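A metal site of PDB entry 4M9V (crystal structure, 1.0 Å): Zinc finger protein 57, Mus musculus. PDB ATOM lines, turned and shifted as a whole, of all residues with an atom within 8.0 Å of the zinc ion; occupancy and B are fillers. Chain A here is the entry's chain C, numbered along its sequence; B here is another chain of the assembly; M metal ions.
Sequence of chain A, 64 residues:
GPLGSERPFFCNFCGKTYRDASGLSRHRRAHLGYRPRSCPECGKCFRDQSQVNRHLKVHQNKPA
N of Glu 41 sits close to SG of Cys 39 (3.3 Å).
OP2 of DT 3 of chain B lies within hydrogen-bond range of a ring nitrogen (ND1) of His 55 (2.9 Å).
The side-chain sulfur (SG) of Cys 42 sits close to the backbone NH (N) of Lys 44, at 3.5 Å.
A ring nitrogen (ND1) of His 59 lies close to the side-chain carboxylate (OE2) of Glu 41 (3.4 Å).
N of Cys 39 lies within hydrogen-bond range of O of Lys 44.
Four residues have an atom within 4 Å of the zinc ion: Cys 39, Cys 42, His 55 and His 59.
The zinc ion is bound by a ring nitrogen (NE2) of His 55 (2.0 Å), a ring nitrogen (NE2) of His 59 (2.0 Å), the side-chain sulfur (SG) of Cys 42 (2.3 Å) and the side-chain sulfur (SG) of Cys 39 (2.3 Å).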
ATOM      1  N   SER A  38      -3.048  15.263   8.866  1.00  0.00           N
ATOM      2  CA  SER A  38      -4.033  14.707   9.768  1.00  0.00           C
ATOM      3  C   SER A  38      -4.242  15.570  10.988  1.00  0.00           C
ATOM      4  O   SER A  38      -3.366  16.336  11.406  1.00  0.00           O
ATOM      5  CB  SER A  38      -3.608  13.325  10.219  1.00  0.00           C
ATOM      6  OG  SER A  38      -2.352  13.399  10.846  1.00  0.00           O
ATOM      7  N   CYS A  39      -5.435  15.435  11.555  1.00  0.00           N
ATOM      8  CA  CYS A  39      -5.769  16.071  12.803  1.00  0.00           C
ATOM      9  C   CYS A  39      -4.975  15.425  13.926  1.00  0.00           C
ATOM     10  O   CYS A  39      -5.009  14.207  14.093  1.00  0.00           O
ATOM     11  CB  CYS A  39      -7.244  15.869  13.088  1.00  0.00           C
ATOM     12  SG  CYS A  39      -7.724  16.580  14.676  1.00  0.00           S
ATOM     13  N   PRO A  40      -4.245  16.226  14.693  1.00  0.00           N
ATOM     14  CA  PRO A  40      -3.442  15.601  15.762  1.00  0.00           C
ATOM     15  C   PRO A  40      -4.302  15.110  16.914  1.00  0.00           C
ATOM     16  O   PRO A  40      -3.860  14.262  17.689  1.00  0.00           O
ATOM     17  CB  PRO A  40      -2.499  16.730  16.194  1.00  0.00           C
ATOM     18  CG  PRO A  40      -3.223  17.977  15.826  1.00  0.00           C
ATOM     19  CD  PRO A  40      -3.981  17.668  14.578  1.00  0.00           C
ATOM     20  N   GLU A  41      -5.534  15.597  17.002  1.00  0.00           N
ATOM     21  CA  GLU A  41      -6.399  15.211  18.103  1.00  0.00           C
ATOM     22  C   GLU A  41      -7.041  13.838  17.847  1.00  0.00           C
ATOM     23  O   GLU A  41      -7.073  13.004  18.758  1.00  0.00           O
ATOM     24  CB  GLU A  41      -7.455  16.283  18.330  1.00  0.00           C
ATOM     25  CG  GLU A  41      -8.078  16.236  19.709  1.00  0.00           C
ATOM     26  CD  GLU A  41      -8.719  14.912  20.002  1.00  0.00           C
ATOM     27  OE1 GLU A  41      -8.471  14.370  21.091  1.00  0.00           O
ATOM     28  OE2 GLU A  41      -9.472  14.418  19.139  1.00  0.00           O
ATOM     29  N   CYS A  42      -7.559  13.608  16.630  1.00  0.00           N
ATOM     30  CA  CYS A  42      -8.300  12.381  16.358  1.00  0.00           C
ATOM     31  C   CYS A  42      -7.751  11.521  15.239  1.00  0.00           C
ATOM     32  O   CYS A  42      -8.215  10.399  15.040  1.00  0.00           O
ATOM     33  CB  CYS A  42      -9.768  12.687  16.057  1.00  0.00           C
ATOM     34  SG  CYS A  42     -10.065  13.493  14.451  1.00  0.00           S
ATOM     35  N   GLY A  43      -6.773  12.044  14.498  1.00  0.00           N
ATOM     36  CA  GLY A  43      -6.141  11.277  13.434  1.00  0.00           C
ATOM     37  C   GLY A  43      -6.833  11.362  12.082  1.00  0.00           C
ATOM     38  O   GLY A  43      -6.307  10.823  11.103  1.00  0.00           O
ATOM     39  N   LYS A  44      -7.983  12.019  11.994  1.00  0.00           N
ATOM     40  CA  LYS A  44      -8.674  12.092  10.711  1.00  0.00           C
ATOM     41  C   LYS A  44      -7.813  12.834   9.697  1.00  0.00           C
ATOM     42  O   LYS A  44      -7.238  13.874   9.999  1.00  0.00           O
ATOM     43  CB  LYS A  44     -10.030  12.779  10.847  1.00  0.00           C
ATOM     44  CG  LYS A  44     -10.838  12.782   9.555  1.00  0.00           C
ATOM     45  CD  LYS A  44     -12.283  13.177   9.755  1.00  0.00           C
ATOM     46  CE  LYS A  44     -13.039  13.167   8.427  1.00  0.00           C
ATOM     47  NZ  LYS A  44     -14.506  13.011   8.594  1.00  0.00           N
ATOM     48  N   CYS A  45      -7.754  12.281   8.482  1.00  0.00           N
ATOM     49  CA  CYS A  45      -6.893  12.831   7.452  1.00  0.00           C
ATOM     50  C   CYS A  45      -7.647  13.744   6.511  1.00  0.00           C
ATOM     51  O   CYS A  45      -8.829  13.543   6.225  1.00  0.00           O
ATOM     52  CB  CYS A  45      -6.228  11.713   6.666  1.00  0.00           C
ATOM     53  SG  CYS A  45      -5.124  10.706   7.663  1.00  0.00           S
ATOM     54  N   PHE A  46      -6.924  14.755   6.025  1.00  0.00           N
ATOM     55  CA  PHE A  46      -7.427  15.762   5.115  1.00  0.00           C
ATOM     56  C   PHE A  46      -6.397  16.050   4.031  1.00  0.00           C
ATOM     57  O   PHE A  46      -5.232  15.631   4.113  1.00  0.00           O
ATOM     58  CB  PHE A  46      -7.793  17.044   5.880  1.00  0.00           C
ATOM     59  CG  PHE A  46      -8.986  16.883   6.778  1.00  0.00           C
ATOM     60  CD1 PHE A  46      -8.830  16.434   8.079  1.00  0.00           C
ATOM     61  CD2 PHE A  46     -10.258  17.141   6.321  1.00  0.00           C
ATOM     62  CE1 PHE A  46      -9.955  16.241   8.890  1.00  0.00           C
ATOM     63  CE2 PHE A  46     -11.374  16.963   7.132  1.00  0.00           C
ATOM     64  CZ  PHE A  46     -11.211  16.509   8.405  1.00  0.00           C
ATOM     65  N   VAL A  52      -7.417  20.513   7.629  1.00  0.00           N
ATOM     66  CA  VAL A  52      -7.267  20.050   9.005  1.00  0.00           C
ATOM     67  C   VAL A  52      -7.681  21.169   9.960  1.00  0.00           C
ATOM     68  O   VAL A  52      -8.464  20.945  10.902  1.00  0.00           O
ATOM     69  CB  VAL A  52      -5.823  19.637   9.351  1.00  0.00           C
ATOM     70  CG1 VAL A  52      -5.684  19.355  10.830  1.00  0.00           C
ATOM     71  CG2 VAL A  52      -5.402  18.414   8.522  1.00  0.00           C
ATOM     72  N   HIS A  55     -11.315  21.656  10.413  1.00  0.00           N
ATOM     73  CA  HIS A  55     -11.876  20.534  11.139  1.00  0.00           C
ATOM     74  C   HIS A  55     -11.717  20.625  12.655  1.00  0.00           C
ATOM     75  O   HIS A  55     -12.526  20.075  13.386  1.00  0.00           O
ATOM     76  CB  HIS A  55     -11.221  19.244  10.614  1.00  0.00           C
ATOM     77  CG  HIS A  55     -11.255  18.105  11.583  1.00  0.00           C
ATOM     78  ND1 HIS A  55     -12.342  17.278  11.769  1.00  0.00           N
ATOM     79  CD2 HIS A  55     -10.326  17.689  12.480  1.00  0.00           C
ATOM     80  CE1 HIS A  55     -12.066  16.391  12.702  1.00  0.00           C
ATOM     81  NE2 HIS A  55     -10.855  16.627  13.182  1.00  0.00           N
ATOM     82  N   LEU A  56     -10.667  21.294  13.121  1.00  0.00           N
ATOM     83  CA  LEU A  56     -10.292  21.216  14.532  1.00  0.00           C
ATOM     84  C   LEU A  56     -11.442  21.571  15.469  1.00  0.00           C
ATOM     85  O   LEU A  56     -11.540  21.005  16.548  1.00  0.00           O
ATOM     86  CB  LEU A  56      -9.113  22.120  14.838  1.00  0.00           C
ATOM     87  CG  LEU A  56      -7.800  21.788  14.110  1.00  0.00           C
ATOM     88  CD1 LEU A  56      -6.794  22.886  14.393  1.00  0.00           C
ATOM     89  CD2 LEU A  56      -7.264  20.423  14.511  1.00  0.00           C
ATOM     90  N   LYS A  57     -12.298  22.518  15.081  1.00  0.00           N
ATOM     91  CA  LYS A  57     -13.368  22.965  15.961  1.00  0.00           C
ATOM     92  C   LYS A  57     -14.339  21.871  16.369  1.00  0.00           C
ATOM     93  O   LYS A  57     -15.068  22.052  17.336  1.00  0.00           O
ATOM     94  CB  LYS A  57     -14.112  24.164  15.375  1.00  0.00           C
ATOM     95  CG  LYS A  57     -14.859  23.860  14.091  1.00  0.00           C
ATOM     96  CD  LYS A  57     -15.615  25.083  13.564  1.00  0.00           C
ATOM     97  CE  LYS A  57     -14.692  26.178  13.069  1.00  0.00           C
ATOM     98  NZ  LYS A  57     -13.971  25.815  11.831  1.00  0.00           N
ATOM     99  N   VAL A  58     -14.353  20.747  15.647  1.00  0.00           N
ATOM    100  CA  VAL A  58     -15.088  19.563  16.089  1.00  0.00           C
ATOM    101  C   VAL A  58     -14.790  19.275  17.565  1.00  0.00           C
ATOM    102  O   VAL A  58     -15.683  18.889  18.325  1.00  0.00           O
ATOM    103  CB  VAL A  58     -14.727  18.316  15.219  1.00  0.00           C
ATOM    104  CG1 VAL A  58     -15.165  17.023  15.885  1.00  0.00           C
ATOM    105  CG2 VAL A  58     -15.336  18.436  13.837  1.00  0.00           C
ATOM    106  N   HIS A  59     -13.549  19.509  17.964  1.00  0.00           N
ATOM    107  CA  HIS A  59     -13.063  19.117  19.293  1.00  0.00           C
ATOM    108  C   HIS A  59     -13.270  20.154  20.384  1.00  0.00           C
ATOM    109  O   HIS A  59     -12.909  19.905  21.534  1.00  0.00           O
ATOM    110  CB  HIS A  59     -11.608  18.711  19.195  1.00  0.00           C
ATOM    111  CG  HIS A  59     -11.368  17.635  18.195  1.00  0.00           C
ATOM    112  ND1 HIS A  59     -12.025  16.417  18.225  1.00  0.00           N
ATOM    113  CD2 HIS A  59     -10.599  17.603  17.076  1.00  0.00           C
ATOM    114  CE1 HIS A  59     -11.648  15.684  17.193  1.00  0.00           C
ATOM    115  NE2 HIS A  59     -10.777  16.374  16.481  1.00  0.00           N
ATOM    116  P    DT B   3     -15.560  16.624   9.734  1.00  0.00           P
ATOM    117  OP1  DT B   3     -15.151  15.220  10.014  1.00  0.00           O
ATOM    118  OP2  DT B   3     -14.702  17.711  10.174  1.00  0.00           O
ATOM    119  O5'  DT B   3     -15.714  16.858   8.186  1.00  0.00           O
ATOM    120  C5'  DT B   3     -16.538  15.994   7.444  1.00  0.00           C
ATOM    121  C4'  DT B   3     -16.635  16.560   6.047  1.00  0.00           C
ATOM    122  O4'  DT B   3     -17.433  17.769   6.025  1.00  0.00           O
ATOM    123  C3'  DT B   3     -15.292  16.941   5.404  1.00  0.00           C
ATOM    124  O3'  DT B   3     -15.291  16.538   4.057  1.00  0.00           O
ATOM    125  C2'  DT B   3     -15.329  18.470   5.411  1.00  0.00           C
ATOM    126  C1'  DT B   3     -16.813  18.677   5.132  1.00  0.00           C
ATOM    127  N1   DT B   3     -17.345  20.030   5.372  1.00  0.00           N
ATOM    128  C2   DT B   3     -18.282  20.499   4.477  1.00  0.00           C
ATOM    129  O2   DT B   3     -18.690  19.856   3.524  1.00  0.00           O
ATOM    130  N3   DT B   3     -18.731  21.759   4.742  1.00  0.00           N
ATOM    131  C4   DT B   3     -18.359  22.579   5.778  1.00  0.00           C
ATOM    132  O4   DT B   3     -18.828  23.703   5.908  1.00  0.00           O
ATOM    133  C5   DT B   3     -17.396  22.025   6.689  1.00  0.00           C
ATOM    134  C7   DT B   3     -16.922  22.844   7.855  1.00  0.00           C
ATOM    135  C6   DT B   3     -16.927  20.801   6.444  1.00  0.00           C
HETATM  136 ZN    ZN M   1      -9.888  15.765  14.747  1.00  0.00          ZN
